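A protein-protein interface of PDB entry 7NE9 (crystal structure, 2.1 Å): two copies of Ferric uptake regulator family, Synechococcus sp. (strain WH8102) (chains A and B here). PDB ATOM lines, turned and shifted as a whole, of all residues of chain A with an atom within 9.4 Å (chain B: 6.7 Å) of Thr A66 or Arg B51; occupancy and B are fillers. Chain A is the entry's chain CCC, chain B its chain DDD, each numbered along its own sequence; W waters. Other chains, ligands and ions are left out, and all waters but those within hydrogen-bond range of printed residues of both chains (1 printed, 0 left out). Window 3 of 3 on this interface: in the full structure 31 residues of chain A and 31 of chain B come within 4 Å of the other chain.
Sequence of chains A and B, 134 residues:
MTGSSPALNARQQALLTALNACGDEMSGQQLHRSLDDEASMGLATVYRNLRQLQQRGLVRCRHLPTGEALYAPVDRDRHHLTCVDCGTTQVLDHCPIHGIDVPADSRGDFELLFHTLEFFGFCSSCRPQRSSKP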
ATOM      1  N   ARG A  62     -32.674 -31.384 -15.685  1.00  0.00           N
ATOM      2  CA  ARG A  62     -32.628 -30.051 -15.049  1.00  0.00           C
ATOM      3  C   ARG A  62     -31.508 -30.059 -14.007  1.00  0.00           C
ATOM      4  O   ARG A  62     -31.060 -31.157 -13.604  1.00  0.00           O
ATOM      5  CB  ARG A  62     -33.991 -29.737 -14.430  1.00  0.00           C
ATOM      6  CG  ARG A  62     -34.309 -30.611 -13.229  1.00  0.00           C
ATOM      7  CD  ARG A  62     -35.672 -30.291 -12.681  1.00  0.00           C
ATOM      8  NE  ARG A  62     -35.893 -31.015 -11.439  1.00  0.00           N
ATOM      9  CZ  ARG A  62     -35.813 -30.487 -10.245  1.00  0.00           C
ATOM     10  NH1 ARG A  62     -35.527 -29.216 -10.089  1.00  0.00           N
ATOM     11  NH2 ARG A  62     -36.030 -31.226  -9.186  1.00  0.00           N
ATOM     12  N   HIS A  63     -31.095 -28.886 -13.562  1.00  0.00           N
ATOM     13  CA  HIS A  63     -29.994 -28.719 -12.593  1.00  0.00           C
ATOM     14  C   HIS A  63     -30.577 -28.190 -11.292  1.00  0.00           C
ATOM     15  O   HIS A  63     -31.356 -27.253 -11.342  1.00  0.00           O
ATOM     16  CB  HIS A  63     -28.919 -27.807 -13.182  1.00  0.00           C
ATOM     17  CG  HIS A  63     -28.173 -28.439 -14.309  1.00  0.00           C
ATOM     18  ND1 HIS A  63     -28.628 -28.377 -15.613  1.00  0.00           N
ATOM     19  CD2 HIS A  63     -27.041 -29.174 -14.332  1.00  0.00           C
ATOM     20  CE1 HIS A  63     -27.790 -29.016 -16.397  1.00  0.00           C
ATOM     21  NE2 HIS A  63     -26.799 -29.506 -15.641  1.00  0.00           N
ATOM     22  N   LEU A  64     -30.152 -28.755 -10.174  1.00  0.00           N
ATOM     23  CA  LEU A  64     -30.369 -28.151  -8.843  1.00  0.00           C
ATOM     24  C   LEU A  64     -29.574 -26.862  -8.757  1.00  0.00           C
ATOM     25  O   LEU A  64     -28.684 -26.631  -9.562  1.00  0.00           O
ATOM     26  CB  LEU A  64     -29.993 -29.160  -7.764  1.00  0.00           C
ATOM     27  CG  LEU A  64     -30.916 -30.384  -7.712  1.00  0.00           C
ATOM     28  CD1 LEU A  64     -30.426 -31.374  -6.670  1.00  0.00           C
ATOM     29  CD2 LEU A  64     -32.383 -29.987  -7.445  1.00  0.00           C
ATOM     30  N   PRO A  65     -29.955 -25.945  -7.844  1.00  0.00           N
ATOM     31  CA  PRO A  65     -29.291 -24.652  -7.735  1.00  0.00           C
ATOM     32  C   PRO A  65     -27.776 -24.782  -7.528  1.00  0.00           C
ATOM     33  O   PRO A  65     -27.102 -23.836  -7.805  1.00  0.00           O
ATOM     34  CB  PRO A  65     -29.975 -24.003  -6.520  1.00  0.00           C
ATOM     35  CG  PRO A  65     -31.358 -24.605  -6.521  1.00  0.00           C
ATOM     36  CD  PRO A  65     -31.139 -26.037  -6.966  1.00  0.00           C
ATOM     37  N   THR A  66     -27.321 -25.883  -6.935  1.00  0.00           N
ATOM     38  CA  THR A  66     -25.894 -26.167  -6.645  1.00  0.00           C
ATOM     39  C   THR A  66     -25.247 -26.955  -7.796  1.00  0.00           C
ATOM     40  O   THR A  66     -24.077 -27.311  -7.650  1.00  0.00           O
ATOM     41  CB  THR A  66     -25.700 -26.936  -5.326  1.00  0.00           C
ATOM     42  OG1 THR A  66     -26.518 -28.103  -5.419  1.00  0.00           O
ATOM     43  CG2 THR A  66     -25.986 -26.085  -4.107  1.00  0.00           C
ATOM     44  N   GLY A  67     -25.934 -27.161  -8.916  1.00  0.00           N
ATOM     45  CA  GLY A  67     -25.294 -27.579 -10.178  1.00  0.00           C
ATOM     46  C   GLY A  67     -25.464 -29.051 -10.487  1.00  0.00           C
ATOM     47  O   GLY A  67     -25.156 -29.441 -11.629  1.00  0.00           O
ATOM     48  N   GLU A  68     -25.997 -29.846  -9.568  1.00  0.00           N
ATOM     49  CA  GLU A  68     -26.244 -31.294  -9.815  1.00  0.00           C
ATOM     50  C   GLU A  68     -27.325 -31.479 -10.891  1.00  0.00           C
ATOM     51  O   GLU A  68     -28.414 -30.866 -10.779  1.00  0.00           O
ATOM     52  CB  GLU A  68     -26.755 -31.998  -8.554  1.00  0.00           C
ATOM     53  CG  GLU A  68     -25.827 -31.926  -7.366  1.00  0.00           C
ATOM     54  CD  GLU A  68     -26.397 -32.436  -6.037  1.00  0.00           C
ATOM     55  OE1 GLU A  68     -27.635 -32.731  -5.911  1.00  0.00           O
ATOM     56  OE2 GLU A  68     -25.587 -32.551  -5.100  1.00  0.00           O
ATOM     57  N   ALA A  69     -27.077 -32.342 -11.866  1.00  0.00           N
ATOM     58  CA  ALA A  69     -28.013 -32.652 -12.959  1.00  0.00           C
ATOM     59  C   ALA A  69     -28.939 -33.790 -12.526  1.00  0.00           C
ATOM     60  O   ALA A  69     -28.469 -34.770 -11.918  1.00  0.00           O
ATOM     61  CB  ALA A  69     -27.244 -32.972 -14.192  1.00  0.00           C
ATOM     62  N   LEU A  70     -30.234 -33.626 -12.785  1.00  0.00           N
ATOM     63  CA  LEU A  70     -31.264 -34.684 -12.559  1.00  0.00           C
ATOM     64  C   LEU A  70     -31.912 -35.042 -13.892  1.00  0.00           C
ATOM     65  O   LEU A  70     -32.253 -34.118 -14.637  1.00  0.00           O
ATOM     66  CB  LEU A  70     -32.325 -34.180 -11.583  1.00  0.00           C
ATOM     67  CG  LEU A  70     -31.816 -33.796 -10.199  1.00  0.00           C
ATOM     68  CD1 LEU A  70     -32.933 -33.227  -9.359  1.00  0.00           C
ATOM     69  CD2 LEU A  70     -31.165 -34.987  -9.518  1.00  0.00           C
ATOM     70  N   THR A  82     -38.630 -24.397  -5.001  1.00  0.00           N
ATOM     71  CA  THR A  82     -37.353 -24.686  -4.310  1.00  0.00           C
ATOM     72  C   THR A  82     -36.951 -23.443  -3.519  1.00  0.00           C
ATOM     73  O   THR A  82     -36.966 -22.335  -4.104  1.00  0.00           O
ATOM     74  CB  THR A  82     -36.273 -25.109  -5.315  1.00  0.00           C
ATOM     75  OG1 THR A  82     -36.806 -26.238  -6.022  1.00  0.00           O
ATOM     76  CG2 THR A  82     -34.974 -25.480  -4.613  1.00  0.00           C
ATOM     77  N   CYS A  83     -36.607 -23.638  -2.251  1.00  0.00           N
ATOM     78  CA  CYS A  83     -36.049 -22.572  -1.397  1.00  0.00           C
ATOM     79  C   CYS A  83     -34.594 -22.324  -1.800  1.00  0.00           C
ATOM     80  O   CYS A  83     -33.809 -23.276  -1.812  1.00  0.00           O
ATOM     81  CB  CYS A  83     -36.152 -22.929   0.074  1.00  0.00           C
ATOM     82  SG  CYS A  83     -35.561 -21.608   1.155  1.00  0.00           S
ATOM     83  N   VAL A  84     -34.262 -21.079  -2.117  1.00  0.00           N
ATOM     84  CA  VAL A  84     -32.902 -20.671  -2.569  1.00  0.00           C
ATOM     85  C   VAL A  84     -31.960 -20.691  -1.364  1.00  0.00           C
ATOM     86  O   VAL A  84     -30.756 -20.693  -1.580  1.00  0.00           O
ATOM     87  CB  VAL A  84     -32.927 -19.279  -3.240  1.00  0.00           C
ATOM     88  CG1 VAL A  84     -33.813 -19.285  -4.467  1.00  0.00           C
ATOM     89  CG2 VAL A  84     -33.336 -18.170  -2.277  1.00  0.00           C
ATOM     90  N   ASP A  85     -32.494 -20.649  -0.142  1.00  0.00           N
ATOM     91  CA  ASP A  85     -31.676 -20.664   1.098  1.00  0.00           C
ATOM     92  C   ASP A  85     -31.324 -22.121   1.457  1.00  0.00           C
ATOM     93  O   ASP A  85     -30.154 -22.482   1.317  1.00  0.00           O
ATOM     94  CB  ASP A  85     -32.390 -19.906   2.220  1.00  0.00           C
ATOM     95  CG  ASP A  85     -31.477 -19.596   3.391  1.00  0.00           C
ATOM     96  OD1 ASP A  85     -30.341 -20.103   3.405  1.00  0.00           O
ATOM     97  OD2 ASP A  85     -31.899 -18.843   4.263  1.00  0.00           O
ATOM     98  N   CYS A  86     -32.295 -22.929   1.882  1.00  0.00           N
ATOM     99  CA  CYS A  86     -32.065 -24.287   2.447  1.00  0.00           C
ATOM    100  C   CYS A  86     -32.193 -25.394   1.387  1.00  0.00           C
ATOM    101  O   CYS A  86     -31.836 -26.537   1.701  1.00  0.00           O
ATOM    102  CB  CYS A  86     -33.028 -24.533   3.600  1.00  0.00           C
ATOM    103  SG  CYS A  86     -34.750 -24.739   3.083  1.00  0.00           S
ATOM    104  N   GLY A  87     -32.672 -25.109   0.176  1.00  0.00           N
ATOM    105  CA  GLY A  87     -32.849 -26.131  -0.876  1.00  0.00           C
ATOM    106  C   GLY A  87     -34.076 -27.024  -0.662  1.00  0.00           C
ATOM    107  O   GLY A  87     -34.285 -27.925  -1.481  1.00  0.00           O
ATOM    108  N   THR A  88     -34.907 -26.820   0.362  1.00  0.00           N
ATOM    109  CA  THR A  88     -36.185 -27.580   0.495  1.00  0.00           C
ATOM    110  C   THR A  88     -37.063 -27.377  -0.749  1.00  0.00           C
ATOM    111  O   THR A  88     -37.052 -26.288  -1.333  1.00  0.00           O
ATOM    112  CB  THR A  88     -36.976 -27.256   1.763  1.00  0.00           C
ATOM    113  OG1 THR A  88     -36.048 -27.582   2.790  1.00  0.00           O
ATOM    114  CG2 THR A  88     -38.207 -28.113   1.928  1.00  0.00           C
ATOM    115  N   PHE A 120     -38.522 -20.520  -7.625  1.00  0.00           N
ATOM    116  CA  PHE A 120     -37.490 -20.278  -6.597  1.00  0.00           C
ATOM    117  C   PHE A 120     -38.028 -19.205  -5.669  1.00  0.00           C
ATOM    118  O   PHE A 120     -38.657 -18.231  -6.138  1.00  0.00           O
ATOM    119  CB  PHE A 120     -36.168 -19.893  -7.266  1.00  0.00           C
ATOM    120  CG  PHE A 120     -35.643 -21.006  -8.124  1.00  0.00           C
ATOM    121  CD1 PHE A 120     -34.988 -22.092  -7.548  1.00  0.00           C
ATOM    122  CD2 PHE A 120     -35.884 -21.023  -9.488  1.00  0.00           C
ATOM    123  CE1 PHE A 120     -34.547 -23.147  -8.332  1.00  0.00           C
ATOM    124  CE2 PHE A 120     -35.419 -22.070 -10.275  1.00  0.00           C
ATOM    125  CZ  PHE A 120     -34.752 -23.125  -9.696  1.00  0.00           C
ATOM    126  N   VAL B  46     -15.233 -14.532  -5.915  1.00  0.00           N
ATOM    127  CA  VAL B  46     -16.401 -14.283  -6.798  1.00  0.00           C
ATOM    128  C   VAL B  46     -17.464 -15.362  -6.518  1.00  0.00           C
ATOM    129  O   VAL B  46     -18.622 -14.999  -6.252  1.00  0.00           O
ATOM    130  CB  VAL B  46     -16.037 -14.224  -8.286  1.00  0.00           C
ATOM    131  CG1 VAL B  46     -17.305 -14.102  -9.124  1.00  0.00           C
ATOM    132  CG2 VAL B  46     -15.114 -13.042  -8.601  1.00  0.00           C
ATOM    133  N   TYR B  47     -17.094 -16.638  -6.584  1.00  0.00           N
ATOM    134  CA  TYR B  47     -18.051 -17.761  -6.418  1.00  0.00           C
ATOM    135  C   TYR B  47     -18.679 -17.700  -5.030  1.00  0.00           C
ATOM    136  O   TYR B  47     -19.902 -17.856  -4.958  1.00  0.00           O
ATOM    137  CB  TYR B  47     -17.372 -19.106  -6.653  1.00  0.00           C
ATOM    138  CG  TYR B  47     -17.155 -19.427  -8.105  1.00  0.00           C
ATOM    139  CD1 TYR B  47     -18.212 -19.454  -9.000  1.00  0.00           C
ATOM    140  CD2 TYR B  47     -15.886 -19.723  -8.575  1.00  0.00           C
ATOM    141  CE1 TYR B  47     -18.004 -19.763 -10.335  1.00  0.00           C
ATOM    142  CE2 TYR B  47     -15.669 -20.086  -9.896  1.00  0.00           C
ATOM    143  CZ  TYR B  47     -16.735 -20.085 -10.779  1.00  0.00           C
ATOM    144  OH  TYR B  47     -16.525 -20.393 -12.084  1.00  0.00           O
ATOM    145  N   ARG B  48     -17.892 -17.449  -3.980  1.00  0.00           N
ATOM    146  CA  ARG B  48     -18.392 -17.449  -2.585  1.00  0.00           C
ATOM    147  C   ARG B  48     -19.430 -16.335  -2.480  1.00  0.00           C
ATOM    148  O   ARG B  48     -20.509 -16.582  -1.903  1.00  0.00           O
ATOM    149  CB  ARG B  48     -17.267 -17.243  -1.567  1.00  0.00           C
ATOM    150  CG  ARG B  48     -17.708 -17.383  -0.117  1.00  0.00           C
ATOM    151  CD  ARG B  48     -16.526 -17.365   0.843  1.00  0.00           C
ATOM    152  NE  ARG B  48     -15.789 -16.101   0.761  1.00  0.00           N
ATOM    153  CZ  ARG B  48     -14.587 -15.900   0.198  1.00  0.00           C
ATOM    154  NH1 ARG B  48     -13.915 -16.890  -0.378  1.00  0.00           N
ATOM    155  NH2 ARG B  48     -14.075 -14.677   0.197  1.00  0.00           N
ATOM    156  N   ASN B  49     -19.124 -15.161  -3.030  1.00  0.00           N
ATOM    157  CA  ASN B  49     -20.017 -13.988  -2.914  1.00  0.00           C
ATOM    158  C   ASN B  49     -21.256 -14.202  -3.782  1.00  0.00           C
ATOM    159  O   ASN B  49     -22.347 -13.824  -3.318  1.00  0.00           O
ATOM    160  CB  ASN B  49     -19.273 -12.692  -3.205  1.00  0.00           C
ATOM    161  CG  ASN B  49     -18.504 -12.247  -1.987  1.00  0.00           C
ATOM    162  OD1 ASN B  49     -19.077 -11.697  -1.078  1.00  0.00           O
ATOM    163  ND2 ASN B  49     -17.227 -12.560  -1.924  1.00  0.00           N
ATOM    164  N   LEU B  50     -21.119 -14.840  -4.941  1.00  0.00           N
ATOM    165  CA  LEU B  50     -22.287 -15.160  -5.793  1.00  0.00           C
ATOM    166  C   LEU B  50     -23.223 -16.087  -5.026  1.00  0.00           C
ATOM    167  O   LEU B  50     -24.413 -15.835  -5.050  1.00  0.00           O
ATOM    168  CB  LEU B  50     -21.853 -15.825  -7.103  1.00  0.00           C
ATOM    169  CG  LEU B  50     -21.404 -14.856  -8.189  1.00  0.00           C
ATOM    170  CD1 LEU B  50     -20.838 -15.633  -9.348  1.00  0.00           C
ATOM    171  CD2 LEU B  50     -22.537 -13.954  -8.631  1.00  0.00           C
ATOM    172  N   ARG B  51     -22.677 -17.124  -4.391  1.00  0.00           N
ATOM    173  CA  ARG B  51     -23.440 -18.132  -3.629  1.00  0.00           C
ATOM    174  C   ARG B  51     -24.221 -17.424  -2.528  1.00  0.00           C
ATOM    175  O   ARG B  51     -25.417 -17.719  -2.387  1.00  0.00           O
ATOM    176  CB  ARG B  51     -22.512 -19.206  -3.073  1.00  0.00           C
ATOM    177  CG  ARG B  51     -23.224 -20.354  -2.371  1.00  0.00           C
ATOM    178  CD  ARG B  51     -24.259 -21.034  -3.259  1.00  0.00           C
ATOM    179  NE  ARG B  51     -24.915 -22.033  -2.426  1.00  0.00           N
ATOM    180  CZ  ARG B  51     -26.179 -22.444  -2.506  1.00  0.00           C
ATOM    181  NH1 ARG B  51     -27.007 -21.954  -3.411  1.00  0.00           N
ATOM    182  NH2 ARG B  51     -26.613 -23.344  -1.644  1.00  0.00           N
ATOM    183  N   GLN B  52     -23.595 -16.491  -1.820  1.00  0.00           N
ATOM    184  CA  GLN B  52     -24.280 -15.721  -0.747  1.00  0.00           C
ATOM    185  C   GLN B  52     -25.428 -14.913  -1.352  1.00  0.00           C
ATOM    186  O   GLN B  52     -26.523 -14.934  -0.766  1.00  0.00           O
ATOM    187  CB  GLN B  52     -23.310 -14.817   0.010  1.00  0.00           C
ATOM    188  CG  GLN B  52     -22.477 -15.579   1.029  1.00  0.00           C
ATOM    189  CD  GLN B  52     -21.195 -14.849   1.383  1.00  0.00           C
ATOM    190  OE1 GLN B  52     -20.931 -13.720   0.947  1.00  0.00           O
ATOM    191  NE2 GLN B  52     -20.362 -15.516   2.170  1.00  0.00           N
ATOM    192  N   LEU B  53     -25.199 -14.236  -2.474  1.00  0.00           N
ATOM    193  CA  LEU B  53     -26.238 -13.402  -3.137  1.00  0.00           C
ATOM    194  C   LEU B  53     -27.382 -14.307  -3.586  1.00  0.00           C
ATOM    195  O   LEU B  53     -28.518 -13.869  -3.519  1.00  0.00           O
ATOM    196  CB  LEU B  53     -25.622 -12.664  -4.326  1.00  0.00           C
ATOM    197  CG  LEU B  53     -24.672 -11.527  -3.941  1.00  0.00           C
ATOM    198  CD1 LEU B  53     -23.930 -10.993  -5.160  1.00  0.00           C
ATOM    199  CD2 LEU B  53     -25.412 -10.400  -3.255  1.00  0.00           C
ATOM    200  N   GLN B  54     -27.073 -15.512  -4.064  1.00  0.00           N
ATOM    201  CA  GLN B  54     -28.093 -16.488  -4.528  1.00  0.00           C
ATOM    202  C   GLN B  54     -28.955 -16.895  -3.331  1.00  0.00           C
ATOM    203  O   GLN B  54     -30.183 -16.927  -3.466  1.00  0.00           O
ATOM    204  CB  GLN B  54     -27.391 -17.690  -5.138  1.00  0.00           C
ATOM    205  CG  GLN B  54     -28.262 -18.614  -5.966  1.00  0.00           C
ATOM    206  CD  GLN B  54     -27.481 -19.847  -6.372  1.00  0.00           C
ATOM    207  OE1 GLN B  54     -26.339 -20.068  -5.956  1.00  0.00           O
ATOM    208  NE2 GLN B  54     -28.133 -20.704  -7.147  1.00  0.00           N
ATOM    209  N   GLN B  55     -28.320 -17.175  -2.200  1.00  0.00           N
ATOM    210  CA  GLN B  55     -29.012 -17.662  -0.978  1.00  0.00           C
ATOM    211  C   GLN B  55     -29.885 -16.550  -0.413  1.00  0.00           C
ATOM    212  O   GLN B  55     -30.934 -16.895   0.185  1.00  0.00           O
ATOM    213  CB  GLN B  55     -28.020 -18.227   0.035  1.00  0.00           C
ATOM    214  CG  GLN B  55     -27.556 -19.597  -0.440  1.00  0.00           C
ATOM    215  CD  GLN B  55     -26.718 -20.308   0.581  1.00  0.00           C
ATOM    216  OE1 GLN B  55     -25.646 -19.853   0.904  1.00  0.00           O
ATOM    217  NE2 GLN B  55     -27.245 -21.383   1.146  1.00  0.00           N
ATOM    218  N   ARG B  56     -29.506 -15.290  -0.627  1.00  0.00           N
ATOM    219  CA  ARG B  56     -30.318 -14.117  -0.198  1.00  0.00           C
ATOM    220  C   ARG B  56     -31.353 -13.761  -1.265  1.00  0.00           C
ATOM    221  O   ARG B  56     -32.062 -12.797  -1.044  1.00  0.00           O
ATOM    222  CB  ARG B  56     -29.406 -12.928   0.088  1.00  0.00           C
ATOM    223  CG  ARG B  56     -28.483 -13.186   1.269  1.00  0.00           C
ATOM    224  CD  ARG B  56     -27.536 -12.044   1.552  1.00  0.00           C
ATOM    225  NE  ARG B  56     -28.240 -10.903   2.107  1.00  0.00           N
ATOM    226  CZ  ARG B  56     -27.672  -9.720   2.335  1.00  0.00           C
ATOM    227  NH1 ARG B  56     -26.393  -9.512   2.056  1.00  0.00           N
ATOM    228  NH2 ARG B  56     -28.382  -8.729   2.842  1.00  0.00           N
ATOM    229  N   VAL B  59     -29.597 -12.522  -6.590  1.00  0.00           N
ATOM    230  CA  VAL B  59     -29.216 -12.919  -7.959  1.00  0.00           C
ATOM    231  C   VAL B  59     -29.986 -14.187  -8.285  1.00  0.00           C
ATOM    232  O   VAL B  59     -30.254 -15.012  -7.379  1.00  0.00           O
ATOM    233  CB  VAL B  59     -27.700 -13.124  -8.129  1.00  0.00           C
ATOM    234  CG1 VAL B  59     -26.924 -11.901  -7.710  1.00  0.00           C
ATOM    235  CG2 VAL B  59     -27.191 -14.359  -7.413  1.00  0.00           C
ATOM    236  N   HIS B  63     -28.737 -22.956 -15.261  1.00  0.00           N
ATOM    237  CA  HIS B  63     -27.645 -23.816 -15.769  1.00  0.00           C
ATOM    238  C   HIS B  63     -27.877 -24.062 -17.249  1.00  0.00           C
ATOM    239  O   HIS B  63     -28.988 -24.375 -17.611  1.00  0.00           O
ATOM    240  CB  HIS B  63     -27.565 -25.092 -14.937  1.00  0.00           C
ATOM    241  CG  HIS B  63     -27.106 -24.834 -13.541  1.00  0.00           C
ATOM    242  ND1 HIS B  63     -27.968 -24.462 -12.521  1.00  0.00           N
ATOM    243  CD2 HIS B  63     -25.883 -24.887 -12.985  1.00  0.00           C
ATOM    244  CE1 HIS B  63     -27.283 -24.289 -11.409  1.00  0.00           C
ATOM    245  NE2 HIS B  63     -26.018 -24.560 -11.655  1.00  0.00           N
ATOM    246  N   TYR B  71     -25.518 -16.264 -14.111  1.00  0.00           N
ATOM    247  CA  TYR B  71     -26.098 -15.402 -13.063  1.00  0.00           C
ATOM    248  C   TYR B  71     -26.631 -14.125 -13.695  1.00  0.00           C
ATOM    249  O   TYR B  71     -26.097 -13.664 -14.692  1.00  0.00           O
ATOM    250  CB  TYR B  71     -25.027 -15.109 -12.014  1.00  0.00           C
ATOM    251  CG  TYR B  71     -24.498 -16.357 -11.357  1.00  0.00           C
ATOM    252  CD1 TYR B  71     -25.100 -16.865 -10.211  1.00  0.00           C
ATOM    253  CD2 TYR B  71     -23.448 -17.071 -11.906  1.00  0.00           C
ATOM    254  CE1 TYR B  71     -24.626 -18.019  -9.595  1.00  0.00           C
ATOM    255  CE2 TYR B  71     -22.979 -18.233 -11.314  1.00  0.00           C
ATOM    256  CZ  TYR B  71     -23.550 -18.693 -10.142  1.00  0.00           C
ATOM    257  OH  TYR B  71     -23.063 -19.816  -9.542  1.00  0.00           O
HETATM  258  O   HOH W   1     -29.893 -21.710  -3.706  1.00  0.00           O
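O of Pro A65 is in hydrogen-bond range of NE2 of Gln B54 (3.4 Å). O of Asp A85 sits at hydrogen-bond distance from NE2 of Gln B55 (3.1 Å).
The side-chain sulfur (SG) of Cys A83 sits close to the backbone NH (N) of Asp A85. The guanidinium group (NH1) of Arg B51 is in hydrogen-bond range of the side-chain amide oxygen (OE1) of Gln B54 (3.2 Å). The guanidinium group (NH2) of Arg B51 lies close to the side-chain amide nitrogen (NE2) of Gln B55, at 3.5 Å.
Among the printed residues, pairs that only touch across the chains: His A63 with His B63, Leu A64 with His B63, Pro A65 with His B63, Thr A66 with Arg B51, Gly A67 with His B63, Val A84 with Gln B54 and Val A84 with Gln B55.
Of chain B, only Arg B51 (3.7 Å) comes within 4 Å of Thr A66. Of chain A, only Thr A66 comes within 4 Å of Arg B51. Of the printed residues of chain B, Asp A85 touches Gln B55. Printed residues of chain B within 4 Å of Leu A64: His B63. Of the printed residues of chain A, His B63 touches His A63 (3.5 Å), Leu A64 (3.3 Å), Pro A65 (3.6 Å) and Gly A67 (3.4 Å). Ala A69 touches none of the printed residues of chain B.
Of the 14 printed residues of chain B, 4 touch a printed residue of chain A. Printed residues of chain A that touch a printed residue of chain B: His A63, Leu A64, Pro A65, Thr A66, Gly A67, Val A84 and Asp A85. Among the printed residues, 9 pairs touch across the chains.
His A63 touches its own counterpart, His B63. Of the 9 pairs that touch across the chains among the printed residues, 1 has its exchanged pair printed and touching as well.
Water W1 bridges the backbone carbonyl oxygen (O) of Val A84 (2.5 Å) and the guanidinium group (NH1) of Arg B51 (2.9 Å).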
